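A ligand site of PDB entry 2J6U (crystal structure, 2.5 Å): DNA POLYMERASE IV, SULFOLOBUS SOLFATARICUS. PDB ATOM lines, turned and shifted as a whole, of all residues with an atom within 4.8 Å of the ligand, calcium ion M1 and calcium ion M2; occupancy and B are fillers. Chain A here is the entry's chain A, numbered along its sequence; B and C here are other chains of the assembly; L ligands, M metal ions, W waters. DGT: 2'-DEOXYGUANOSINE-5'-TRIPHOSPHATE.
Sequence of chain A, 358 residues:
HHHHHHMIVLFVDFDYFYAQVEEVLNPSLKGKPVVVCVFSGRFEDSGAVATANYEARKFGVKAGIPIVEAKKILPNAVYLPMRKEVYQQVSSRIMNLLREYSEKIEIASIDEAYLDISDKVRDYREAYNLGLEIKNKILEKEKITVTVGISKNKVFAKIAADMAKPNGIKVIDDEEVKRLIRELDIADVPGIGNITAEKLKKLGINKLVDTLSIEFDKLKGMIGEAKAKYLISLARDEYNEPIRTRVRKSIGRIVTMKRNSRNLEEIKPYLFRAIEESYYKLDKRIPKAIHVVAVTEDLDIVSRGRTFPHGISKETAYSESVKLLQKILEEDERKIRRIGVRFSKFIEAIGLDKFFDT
An oxygen (O3G) of the ligand lies within hydrogen-bond range of the backbone NH (N) of Tyr 16 (2.5 Å).
The side-chain amino group (NZ) of Lys 165 lies within salt-bridge range of an oxygen (O1G) of the ligand, at 3.8 Å.
OG1 of Thr 51 lies within hydrogen-bond range of O2B of the ligand, 2.5 Å away.
N2 of the ligand sits at hydrogen-bond distance from O2 of DC 4 of chain B, at 2.5 Å.
O1G of the ligand is in salt-bridge range of NH1 of Arg 57, 2.7 Å away.
The side-chain hydroxyl (OH) of Tyr 54 is in hydrogen-bond range of an oxygen (O1G) of the ligand (3.1 Å).
An oxygen (O1B) of the ligand lies close to the backbone NH (N) of Phe 17, 3.1 Å away.
N of Tyr 18 sits at hydrogen-bond distance from O3' of the ligand (3.2 Å).
N1 of 6OG 5 of chain B is in hydrogen-bond range of a nitrogen (N1) of the ligand (3.3 Å).
NZ of Lys 165 lies close to OD1 of Asp 13, 3.1 Å away.
NH2 of Arg 57 sits at hydrogen-bond distance from OG1 of Thr 51, 3.4 Å away.
The side-chain hydroxyl (OG) of Ser 109 sits at hydrogen-bond distance from the side-chain carboxylate (OD1) of Asp 111, 3.3 Å away.
The guanidinium group (NH2) of Arg 57 sits at hydrogen-bond distance from the backbone carbonyl oxygen (O) of Ala 52, 2.9 Å away.
Asp 15 touches the ligand (C to O3G, 3.5 Å).
Ala 50 touches the ligand.
DT 14 of chain C touches the ligand.
Hydrophobic or aromatic side chains that line the ligand: Tyr 16, Phe 17, Tyr 18, Ala 50 and Tyr 54.
Of the 24 residues printed, 15 come within 4 Å of the ligand.
Along chain A the residues within 4 Å of the ligand span positions 13 to 165.
OP1 of DT 14 of chain C touches calcium ion M1, at 3.7 Å.
Within 4 Å of calcium ion M1: Asp 13, Asp 111, Glu 112 and DT 14 of chain C.
Within 4 Å of calcium ion M2: Asp 13, Phe 14 of chain A and Asp 111.
Calcium ion M1 is bound by OD2 of Asp 13, 2.6 Å away.
Calcium ion M1 is bound by water W6.
OE2 of Glu 112 binds calcium ion M1 (2.6 Å).
The side-chain carboxylate (OD1) of Asp 13 is bound to calcium ion M1.
An oxygen (O2A) of the ligand binds calcium ion M1 (2.8 Å).
Slightly farther from calcium ion M1 lies OD1 of Asp 111 (3.0 Å).
Calcium ion M2 is bound by an oxygen (O2A) of the ligand (2.3 Å), the backbone carbonyl oxygen of Phe 14 of chain A (2.5 Å), an oxygen (O2G) of the ligand (2.5 Å), the side-chain carboxylate of Asp 13 (2.6 Å), an oxygen (O1B) of the ligand (2.6 Å), the side-chain carboxylate of Asp 111 (2.6 Å) and water W4 (2.9 Å).
Calcium ion M2 has seven donor atoms within binding distance.
Water W6 lies within hydrogen-bond range of OP1 of DT 14 of chain C (2.5 Å), the side-chain amino group of Lys 165 (3.2 Å) and an oxygen (O1A) of the ligand (3.3 Å).
Water W4 bridges the backbone carbonyl oxygen of Asp 13 (2.8 Å) and the side-chain carboxylate of Asp 15 (3.4 Å).
Water W5 lies within hydrogen-bond range of the side-chain amino group (NZ) of Lys 165 (2.5 Å) and an oxygen (O1A) of the ligand (2.5 Å).
Water W1 bridges N3 of DT 14 of chain C (2.5 Å) and N7 of the ligand (2.6 Å).
Water W3 lies within hydrogen-bond range of OH of Tyr 54 (2.9 Å), O1G of the ligand (3.0 Å) and NH1 of Arg 57 (3.4 Å).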
ATOM      1  N   ASP A  13       3.080  15.392 -22.357  1.00  0.00           N
ATOM      2  CA  ASP A  13       1.866  15.560 -21.580  1.00  0.00           C
ATOM      3  C   ASP A  13       1.570  17.054 -21.435  1.00  0.00           C
ATOM      4  O   ASP A  13       2.353  17.785 -20.831  1.00  0.00           O
ATOM      5  CB  ASP A  13       2.083  14.914 -20.204  1.00  0.00           C
ATOM      6  CG  ASP A  13       0.786  14.694 -19.455  1.00  0.00           C
ATOM      7  OD1 ASP A  13       0.834  14.005 -18.392  1.00  0.00           O
ATOM      8  OD2 ASP A  13      -0.233  15.205 -19.955  1.00  0.00           O
ATOM      9  N   PHE A  14       0.440  17.505 -21.972  1.00  0.00           N
ATOM     10  CA  PHE A  14       0.097  18.933 -21.945  1.00  0.00           C
ATOM     11  C   PHE A  14      -0.231  19.458 -20.537  1.00  0.00           C
ATOM     12  O   PHE A  14      -1.100  18.922 -19.873  1.00  0.00           O
ATOM     13  CB  PHE A  14      -1.107  19.243 -22.851  1.00  0.00           C
ATOM     14  CG  PHE A  14      -1.088  18.524 -24.179  1.00  0.00           C
ATOM     15  CD1 PHE A  14       0.090  18.008 -24.716  1.00  0.00           C
ATOM     16  CD2 PHE A  14      -2.268  18.383 -24.904  1.00  0.00           C
ATOM     17  CE1 PHE A  14       0.087  17.364 -25.960  1.00  0.00           C
ATOM     18  CE2 PHE A  14      -2.281  17.749 -26.150  1.00  0.00           C
ATOM     19  CZ  PHE A  14      -1.099  17.239 -26.680  1.00  0.00           C
ATOM     20  N   ASP A  15       0.439  20.511 -20.112  1.00  0.00           N
ATOM     21  CA  ASP A  15       0.213  21.093 -18.785  1.00  0.00           C
ATOM     22  C   ASP A  15      -1.239  21.530 -18.551  1.00  0.00           C
ATOM     23  O   ASP A  15      -1.834  22.211 -19.370  1.00  0.00           O
ATOM     24  CB  ASP A  15       1.146  22.290 -18.571  1.00  0.00           C
ATOM     25  CG  ASP A  15       2.613  21.930 -18.819  1.00  0.00           C
ATOM     26  OD1 ASP A  15       3.016  20.801 -18.451  1.00  0.00           O
ATOM     27  OD2 ASP A  15       3.359  22.775 -19.362  1.00  0.00           O
ATOM     28  N   TYR A  16      -1.784  21.117 -17.394  1.00  0.00           N
ATOM     29  CA  TYR A  16      -3.172  21.410 -16.973  1.00  0.00           C
ATOM     30  C   TYR A  16      -4.085  21.720 -18.166  1.00  0.00           C
ATOM     31  O   TYR A  16      -4.775  22.734 -18.217  1.00  0.00           O
ATOM     32  CB  TYR A  16      -3.159  22.543 -15.962  1.00  0.00           C
ATOM     33  CG  TYR A  16      -2.610  23.840 -16.489  1.00  0.00           C
ATOM     34  CD1 TYR A  16      -3.463  24.872 -16.905  1.00  0.00           C
ATOM     35  CD2 TYR A  16      -1.226  24.061 -16.541  1.00  0.00           C
ATOM     36  CE1 TYR A  16      -2.945  26.098 -17.357  1.00  0.00           C
ATOM     37  CE2 TYR A  16      -0.698  25.269 -16.985  1.00  0.00           C
ATOM     38  CZ  TYR A  16      -1.560  26.287 -17.385  1.00  0.00           C
ATOM     39  OH  TYR A  16      -1.036  27.495 -17.812  1.00  0.00           O
ATOM     40  N   PHE A  17      -4.110  20.776 -19.091  1.00  0.00           N
ATOM     41  CA  PHE A  17      -4.808  20.908 -20.353  1.00  0.00           C
ATOM     42  C   PHE A  17      -6.103  21.689 -20.488  1.00  0.00           C
ATOM     43  O   PHE A  17      -6.094  22.755 -21.086  1.00  0.00           O
ATOM     44  CB  PHE A  17      -4.970  19.549 -21.021  1.00  0.00           C
ATOM     45  CG  PHE A  17      -5.213  19.654 -22.484  1.00  0.00           C
ATOM     46  CD1 PHE A  17      -4.561  20.619 -23.244  1.00  0.00           C
ATOM     47  CD2 PHE A  17      -6.101  18.802 -23.126  1.00  0.00           C
ATOM     48  CE1 PHE A  17      -4.789  20.748 -24.609  1.00  0.00           C
ATOM     49  CE2 PHE A  17      -6.346  18.923 -24.500  1.00  0.00           C
ATOM     50  CZ  PHE A  17      -5.681  19.896 -25.233  1.00  0.00           C
ATOM     51  N   TYR A  18      -7.218  21.180 -19.972  1.00  0.00           N
ATOM     52  CA  TYR A  18      -8.488  21.887 -20.108  1.00  0.00           C
ATOM     53  C   TYR A  18      -8.411  23.340 -19.643  1.00  0.00           C
ATOM     54  O   TYR A  18      -8.972  24.241 -20.287  1.00  0.00           O
ATOM     55  CB  TYR A  18      -9.604  21.176 -19.361  1.00  0.00           C
ATOM     56  CG  TYR A  18      -9.987  19.823 -19.921  1.00  0.00           C
ATOM     57  CD1 TYR A  18      -9.184  19.178 -20.856  1.00  0.00           C
ATOM     58  CD2 TYR A  18     -11.135  19.166 -19.466  1.00  0.00           C
ATOM     59  CE1 TYR A  18      -9.504  17.918 -21.330  1.00  0.00           C
ATOM     60  CE2 TYR A  18     -11.464  17.901 -19.930  1.00  0.00           C
ATOM     61  CZ  TYR A  18     -10.644  17.280 -20.867  1.00  0.00           C
ATOM     62  OH  TYR A  18     -10.941  16.011 -21.306  1.00  0.00           O
ATOM     63  N   VAL A  38     -17.579  20.510 -14.017  1.00  0.00           N
ATOM     64  CA  VAL A  38     -18.548  19.595 -14.571  1.00  0.00           C
ATOM     65  C   VAL A  38     -19.825  19.702 -13.722  1.00  0.00           C
ATOM     66  O   VAL A  38     -19.980  18.998 -12.730  1.00  0.00           O
ATOM     67  CB  VAL A  38     -18.012  18.143 -14.577  1.00  0.00           C
ATOM     68  CG1 VAL A  38     -18.978  17.230 -15.362  1.00  0.00           C
ATOM     69  CG2 VAL A  38     -16.624  18.112 -15.216  1.00  0.00           C
ATOM     70  N   VAL A  49     -14.755  19.138 -10.219  1.00  0.00           N
ATOM     71  CA  VAL A  49     -13.747  19.846 -10.979  1.00  0.00           C
ATOM     72  C   VAL A  49     -13.101  18.880 -11.947  1.00  0.00           C
ATOM     73  O   VAL A  49     -12.667  17.805 -11.542  1.00  0.00           O
ATOM     74  CB  VAL A  49     -12.668  20.439 -10.045  1.00  0.00           C
ATOM     75  CG1 VAL A  49     -11.551  21.052 -10.857  1.00  0.00           C
ATOM     76  CG2 VAL A  49     -13.295  21.478  -9.131  1.00  0.00           C
ATOM     77  N   ALA A  50     -13.028  19.230 -13.221  1.00  0.00           N
ATOM     78  CA  ALA A  50     -12.385  18.339 -14.189  1.00  0.00           C
ATOM     79  C   ALA A  50     -10.869  18.521 -14.068  1.00  0.00           C
ATOM     80  O   ALA A  50     -10.098  17.574 -14.234  1.00  0.00           O
ATOM     81  CB  ALA A  50     -12.848  18.656 -15.620  1.00  0.00           C
ATOM     82  N   THR A  51     -10.467  19.745 -13.747  1.00  0.00           N
ATOM     83  CA  THR A  51      -9.059  20.099 -13.590  1.00  0.00           C
ATOM     84  C   THR A  51      -8.965  21.586 -13.263  1.00  0.00           C
ATOM     85  O   THR A  51      -9.949  22.318 -13.403  1.00  0.00           O
ATOM     86  CB  THR A  51      -8.270  19.834 -14.900  1.00  0.00           C
ATOM     87  OG1 THR A  51      -6.871  19.992 -14.669  1.00  0.00           O
ATOM     88  CG2 THR A  51      -8.711  20.792 -15.978  1.00  0.00           C
ATOM     89  N   ALA A  52      -7.799  22.053 -12.854  1.00  0.00           N
ATOM     90  CA  ALA A  52      -7.612  23.460 -12.524  1.00  0.00           C
ATOM     91  C   ALA A  52      -6.178  23.835 -12.842  1.00  0.00           C
ATOM     92  O   ALA A  52      -5.331  22.956 -12.955  1.00  0.00           O
ATOM     93  CB  ALA A  52      -7.930  23.702 -11.044  1.00  0.00           C
ATOM     94  N   TYR A  54      -2.399  25.555 -12.076  1.00  0.00           N
ATOM     95  CA  TYR A  54      -1.542  25.575 -10.906  1.00  0.00           C
ATOM     96  C   TYR A  54      -1.803  26.697  -9.924  1.00  0.00           C
ATOM     97  O   TYR A  54      -1.597  26.521  -8.737  1.00  0.00           O
ATOM     98  CB  TYR A  54      -0.063  25.566 -11.322  1.00  0.00           C
ATOM     99  CG  TYR A  54       0.361  24.217 -11.834  1.00  0.00           C
ATOM    100  CD1 TYR A  54       0.154  23.863 -13.160  1.00  0.00           C
ATOM    101  CD2 TYR A  54       0.881  23.258 -10.963  1.00  0.00           C
ATOM    102  CE1 TYR A  54       0.461  22.583 -13.623  1.00  0.00           C
ATOM    103  CE2 TYR A  54       1.198  21.981 -11.405  1.00  0.00           C
ATOM    104  CZ  TYR A  54       0.986  21.651 -12.733  1.00  0.00           C
ATOM    105  OH  TYR A  54       1.285  20.371 -13.161  1.00  0.00           O
ATOM    106  N   ARG A  57      -4.440  25.145  -8.040  1.00  0.00           N
ATOM    107  CA  ARG A  57      -4.025  23.848  -7.563  1.00  0.00           C
ATOM    108  C   ARG A  57      -3.145  23.931  -6.328  1.00  0.00           C
ATOM    109  O   ARG A  57      -3.112  23.013  -5.518  1.00  0.00           O
ATOM    110  CB  ARG A  57      -3.291  23.104  -8.675  1.00  0.00           C
ATOM    111  CG  ARG A  57      -3.217  21.598  -8.470  1.00  0.00           C
ATOM    112  CD  ARG A  57      -2.617  20.871  -9.667  1.00  0.00           C
ATOM    113  NE  ARG A  57      -3.429  20.959 -10.878  1.00  0.00           N
ATOM    114  CZ  ARG A  57      -3.121  20.338 -12.013  1.00  0.00           C
ATOM    115  NH1 ARG A  57      -2.022  19.601 -12.072  1.00  0.00           N
ATOM    116  NH2 ARG A  57      -3.890  20.454 -13.090  1.00  0.00           N
ATOM    117  N   ALA A  63      -8.576  18.289  -9.795  1.00  0.00           N
ATOM    118  CA  ALA A  63      -9.526  17.347 -10.369  1.00  0.00           C
ATOM    119  C   ALA A  63     -10.085  16.407  -9.332  1.00  0.00           C
ATOM    120  O   ALA A  63      -9.343  15.880  -8.500  1.00  0.00           O
ATOM    121  CB  ALA A  63      -8.877  16.546 -11.483  1.00  0.00           C
ATOM    122  N   GLY A  64     -11.396  16.198  -9.352  1.00  0.00           N
ATOM    123  CA  GLY A  64     -12.021  15.285  -8.407  1.00  0.00           C
ATOM    124  C   GLY A  64     -12.793  15.882  -7.239  1.00  0.00           C
ATOM    125  O   GLY A  64     -13.665  15.214  -6.684  1.00  0.00           O
ATOM    126  N   MET A  82     -16.822  22.809 -18.364  1.00  0.00           N
ATOM    127  CA  MET A  82     -16.024  22.029 -19.277  1.00  0.00           C
ATOM    128  C   MET A  82     -16.541  22.075 -20.717  1.00  0.00           C
ATOM    129  O   MET A  82     -17.742  21.880 -20.960  1.00  0.00           O
ATOM    130  CB  MET A  82     -15.984  20.566 -18.813  1.00  0.00           C
ATOM    131  CG  MET A  82     -15.223  19.651 -19.753  1.00  0.00           C
ATOM    132  SD  MET A  82     -15.077  18.007 -19.087  1.00  0.00           S
ATOM    133  CE  MET A  82     -16.719  17.355 -19.443  1.00  0.00           C
ATOM    134  N   SER A 109      -4.051   9.383 -24.643  1.00  0.00           N
ATOM    135  CA  SER A 109      -5.209  10.044 -24.047  1.00  0.00           C
ATOM    136  C   SER A 109      -5.398  11.390 -24.708  1.00  0.00           C
ATOM    137  O   SER A 109      -4.671  11.731 -25.655  1.00  0.00           O
ATOM    138  CB  SER A 109      -5.005  10.221 -22.539  1.00  0.00           C
ATOM    139  OG  SER A 109      -4.311  11.425 -22.232  1.00  0.00           O
ATOM    140  N   ILE A 110      -6.356  12.161 -24.212  1.00  0.00           N
ATOM    141  CA  ILE A 110      -6.636  13.462 -24.793  1.00  0.00           C
ATOM    142  C   ILE A 110      -5.505  14.475 -24.705  1.00  0.00           C
ATOM    143  O   ILE A 110      -5.547  15.461 -25.421  1.00  0.00           O
ATOM    144  CB  ILE A 110      -7.937  14.100 -24.202  1.00  0.00           C
ATOM    145  CG1 ILE A 110      -8.454  15.162 -25.184  1.00  0.00           C
ATOM    146  CG2 ILE A 110      -7.678  14.728 -22.796  1.00  0.00           C
ATOM    147  CD1 ILE A 110      -9.781  15.743 -24.801  1.00  0.00           C
ATOM    148  N   ASP A 111      -4.503  14.261 -23.858  1.00  0.00           N
ATOM    149  CA  ASP A 111      -3.426  15.256 -23.806  1.00  0.00           C
ATOM    150  C   ASP A 111      -2.028  14.647 -23.615  1.00  0.00           C
ATOM    151  O   ASP A 111      -1.094  15.312 -23.142  1.00  0.00           O
ATOM    152  CB  ASP A 111      -3.669  16.243 -22.671  1.00  0.00           C
ATOM    153  CG  ASP A 111      -3.290  15.655 -21.345  1.00  0.00           C
ATOM    154  OD1 ASP A 111      -3.420  14.405 -21.252  1.00  0.00           O
ATOM    155  OD2 ASP A 111      -2.861  16.402 -20.427  1.00  0.00           O
ATOM    156  N   GLU A 112      -1.861  13.378 -23.968  1.00  0.00           N
ATOM    157  CA  GLU A 112      -0.541  12.769 -23.855  1.00  0.00           C
ATOM    158  C   GLU A 112      -0.308  11.816 -25.010  1.00  0.00           C
ATOM    159  O   GLU A 112      -1.257  11.345 -25.640  1.00  0.00           O
ATOM    160  CB  GLU A 112      -0.355  12.074 -22.492  1.00  0.00           C
ATOM    161  CG  GLU A 112      -1.070  10.756 -22.282  1.00  0.00           C
ATOM    162  CD  GLU A 112      -0.973  10.280 -20.820  1.00  0.00           C
ATOM    163  OE1 GLU A 112      -0.968   9.051 -20.559  1.00  0.00           O
ATOM    164  OE2 GLU A 112      -0.905  11.131 -19.922  1.00  0.00           O
ATOM    165  N   LYS A 165       6.773  17.960 -14.274  1.00  0.00           N
ATOM    166  CA  LYS A 165       5.602  18.810 -14.427  1.00  0.00           C
ATOM    167  C   LYS A 165       5.683  19.985 -13.464  1.00  0.00           C
ATOM    168  O   LYS A 165       6.115  19.840 -12.319  1.00  0.00           O
ATOM    169  CB  LYS A 165       4.304  18.054 -14.127  1.00  0.00           C
ATOM    170  CG  LYS A 165       3.905  16.984 -15.111  1.00  0.00           C
ATOM    171  CD  LYS A 165       2.540  16.430 -14.754  1.00  0.00           C
ATOM    172  CE  LYS A 165       2.125  15.333 -15.707  1.00  0.00           C
ATOM    173  NZ  LYS A 165       0.722  14.895 -15.459  1.00  0.00           N
ATOM    174  P    DC B   4     -21.694  14.087  -9.068  1.00  0.00           P
ATOM    175  OP1  DC B   4     -22.936  13.432  -8.570  1.00  0.00           O
ATOM    176  OP2  DC B   4     -20.515  13.258  -9.404  1.00  0.00           O
ATOM    177  O5'  DC B   4     -22.081  14.984 -10.347  1.00  0.00           O
ATOM    178  C5'  DC B   4     -21.062  15.706 -11.039  1.00  0.00           C
ATOM    179  C4'  DC B   4     -20.269  14.801 -11.936  1.00  0.00           C
ATOM    180  O4'  DC B   4     -18.853  15.034 -11.790  1.00  0.00           O
ATOM    181  C3'  DC B   4     -20.458  14.731 -13.453  1.00  0.00           C
ATOM    182  O3'  DC B   4     -21.686  14.182 -13.900  1.00  0.00           O
ATOM    183  C2'  DC B   4     -19.244  13.888 -13.829  1.00  0.00           C
ATOM    184  C1'  DC B   4     -18.204  14.627 -12.998  1.00  0.00           C
ATOM    185  N1   DC B   4     -16.968  13.940 -12.614  1.00  0.00           N
ATOM    186  C2   DC B   4     -15.868  14.050 -13.463  1.00  0.00           C
ATOM    187  O2   DC B   4     -16.041  14.537 -14.587  1.00  0.00           O
ATOM    188  N3   DC B   4     -14.657  13.627 -13.043  1.00  0.00           N
ATOM    189  C4   DC B   4     -14.537  13.061 -11.837  1.00  0.00           C
ATOM    190  N4   DC B   4     -13.307  12.730 -11.430  1.00  0.00           N
ATOM    191  C5   DC B   4     -15.670  12.835 -10.991  1.00  0.00           C
ATOM    192  C6   DC B   4     -16.855  13.288 -11.423  1.00  0.00           C
ATOM    193  P   6OG B   5     -22.078  14.258 -15.458  1.00  0.00           P
ATOM    194  OP1 6OG B   5     -22.214  15.654 -15.922  1.00  0.00           O
ATOM    195  OP2 6OG B   5     -23.206  13.320 -15.664  1.00  0.00           O
ATOM    196  O5' 6OG B   5     -20.781  13.695 -16.234  1.00  0.00           O
ATOM    197  N9  6OG B   5     -17.026  11.526 -16.052  1.00  0.00           N
ATOM    198  C4  6OG B   5     -15.696  11.435 -15.982  1.00  0.00           C
ATOM    199  N3  6OG B   5     -14.719  11.760 -16.835  1.00  0.00           N
ATOM    200  C2  6OG B   5     -13.434  11.596 -16.508  1.00  0.00           C
ATOM    201  N2  6OG B   5     -12.504  11.960 -17.390  1.00  0.00           N
ATOM    202  N1  6OG B   5     -13.097  11.090 -15.304  1.00  0.00           N
ATOM    203  C6  6OG B   5     -14.045  10.739 -14.421  1.00  0.00           C
ATOM    204  O6  6OG B   5     -13.660  10.269 -13.205  1.00  0.00           O
ATOM    205  C5  6OG B   5     -15.394  10.914 -14.744  1.00  0.00           C
ATOM    206  N7  6OG B   5     -16.537  10.694 -14.108  1.00  0.00           N
ATOM    207  C8  6OG B   5     -17.534  11.066 -14.911  1.00  0.00           C
ATOM    208  C2' 6OG B   5     -19.127  11.414 -17.475  1.00  0.00           C
ATOM    209  C5' 6OG B   5     -20.240  14.479 -17.294  1.00  0.00           C
ATOM    210  C4' 6OG B   5     -19.142  13.741 -18.006  1.00  0.00           C
ATOM    211  O4' 6OG B   5     -18.111  13.451 -17.046  1.00  0.00           O
ATOM    212  C1' 6OG B   5     -17.774  12.057 -17.211  1.00  0.00           C
ATOM    213  C3' 6OG B   5     -19.551  12.383 -18.573  1.00  0.00           C
ATOM    214  O3' 6OG B   5     -18.841  12.135 -19.788  1.00  0.00           O
ATOM    215  C   6OG B   5     -14.647   9.393 -12.654  1.00  0.00           C
ATOM    216  P    DT C  14      -2.609   9.396 -16.276  1.00  0.00           P
ATOM    217  OP1  DT C  14      -2.934  10.789 -16.630  1.00  0.00           O
ATOM    218  OP2  DT C  14      -1.752   8.600 -17.199  1.00  0.00           O
ATOM    219  O5'  DT C  14      -1.996   9.377 -14.790  1.00  0.00           O
ATOM    220  C5'  DT C  14      -2.390  10.405 -13.875  1.00  0.00           C
ATOM    221  C4'  DT C  14      -1.754  10.231 -12.498  1.00  0.00           C
ATOM    222  O4'  DT C  14      -1.835  11.492 -11.810  1.00  0.00           O
ATOM    223  C3'  DT C  14      -2.417   9.199 -11.592  1.00  0.00           C
ATOM    224  O3'  DT C  14      -1.549   8.696 -10.589  1.00  0.00           O
ATOM    225  C2'  DT C  14      -3.418  10.037 -10.822  1.00  0.00           C
ATOM    226  C1'  DT C  14      -2.764  11.410 -10.737  1.00  0.00           C
ATOM    227  N1   DT C  14      -3.715  12.533 -10.890  1.00  0.00           N
ATOM    228  C2   DT C  14      -4.427  12.595 -12.061  1.00  0.00           C
ATOM    229  O2   DT C  14      -4.346  11.740 -12.924  1.00  0.00           O
ATOM    230  N3   DT C  14      -5.226  13.707 -12.190  1.00  0.00           N
ATOM    231  C4   DT C  14      -5.426  14.705 -11.277  1.00  0.00           C
ATOM    232  O4   DT C  14      -6.161  15.653 -11.547  1.00  0.00           O
ATOM    233  C5   DT C  14      -4.705  14.545 -10.022  1.00  0.00           C
ATOM    234  C7   DT C  14      -4.918  15.548  -8.934  1.00  0.00           C
ATOM    235  C6   DT C  14      -3.886  13.487  -9.905  1.00  0.00           C
HETATM  236  PG  DGT L   1      -1.088  18.137 -15.211  1.00  0.00           P
HETATM  237  O1G DGT L   1      -0.564  17.950 -13.694  1.00  0.00           O
HETATM  238  O2G DGT L   1      -0.232  17.108 -16.094  1.00  0.00           O
HETATM  239  O3G DGT L   1      -0.965  19.536 -15.673  1.00  0.00           O
HETATM  240  O3B DGT L   1      -2.594  17.589 -15.238  1.00  0.00           O
HETATM  241  PB  DGT L   1      -3.711  18.189 -16.228  1.00  0.00           P
HETATM  242  O1B DGT L   1      -3.530  18.069 -17.687  1.00  0.00           O
HETATM  243  O2B DGT L   1      -4.735  19.060 -15.611  1.00  0.00           O
HETATM  244  O3A DGT L   1      -4.467  16.798 -15.963  1.00  0.00           O
HETATM  245  PA  DGT L   1      -4.141  15.451 -16.783  1.00  0.00           P
HETATM  246  O1A DGT L   1      -4.096  14.272 -15.705  1.00  0.00           O
HETATM  247  O2A DGT L   1      -2.894  15.503 -17.568  1.00  0.00           O
HETATM  248  O5' DGT L   1      -5.463  15.240 -17.690  1.00  0.00           O
HETATM  249  C5' DGT L   1      -5.696  16.073 -18.832  1.00  0.00           C
HETATM  250  C4' DGT L   1      -7.153  16.513 -18.895  1.00  0.00           C
HETATM  251  O4' DGT L   1      -8.055  15.406 -18.759  1.00  0.00           O
HETATM  252  C3' DGT L   1      -7.470  17.375 -17.672  1.00  0.00           C
HETATM  253  O3' DGT L   1      -6.971  18.699 -17.891  1.00  0.00           O
HETATM  254  C2' DGT L   1      -8.983  17.379 -17.828  1.00  0.00           C
HETATM  255  C1' DGT L   1      -9.236  15.890 -18.080  1.00  0.00           C
HETATM  256  N9  DGT L   1      -9.342  15.170 -16.780  1.00  0.00           N
HETATM  257  C8  DGT L   1      -8.357  14.687 -16.040  1.00  0.00           C
HETATM  258  N7  DGT L   1      -8.877  14.131 -14.943  1.00  0.00           N
HETATM  259  C5  DGT L   1     -10.202  14.262 -14.977  1.00  0.00           C
HETATM  260  C6  DGT L   1     -11.209  13.885 -14.107  1.00  0.00           C
HETATM  261  O6  DGT L   1     -10.964  13.328 -13.032  1.00  0.00           O
HETATM  262  N1  DGT L   1     -12.527  14.203 -14.477  1.00  0.00           N
HETATM  263  C2  DGT L   1     -12.779  14.883 -15.672  1.00  0.00           C
HETATM  264  N2  DGT L   1     -14.029  15.170 -16.019  1.00  0.00           N
HETATM  265  N3  DGT L   1     -11.771  15.225 -16.487  1.00  0.00           N
HETATM  266  C4  DGT L   1     -10.499  14.932 -16.165  1.00  0.00           C
HETATM  267 CA    CA M   1      -1.738  13.413 -18.938  1.00  0.00          CA
HETATM  268 CA    CA M   2      -1.288  16.959 -18.373  1.00  0.00          CA
HETATM  269  O   HOH W   1      -7.556  13.135 -12.892  1.00  0.00           O
HETATM  270  O   HOH W   2      -9.761  12.470 -10.587  1.00  0.00           O
HETATM  271  O   HOH W   3       1.025  18.283 -11.205  1.00  0.00           O
HETATM  272  O   HOH W   4       1.465  17.733 -18.199  1.00  0.00           O
HETATM  273  O   HOH W   5      -1.739  14.967 -15.358  1.00  0.00           O
HETATM  274  O   HOH W   6      -1.301  12.679 -16.524  1.00  0.00           O
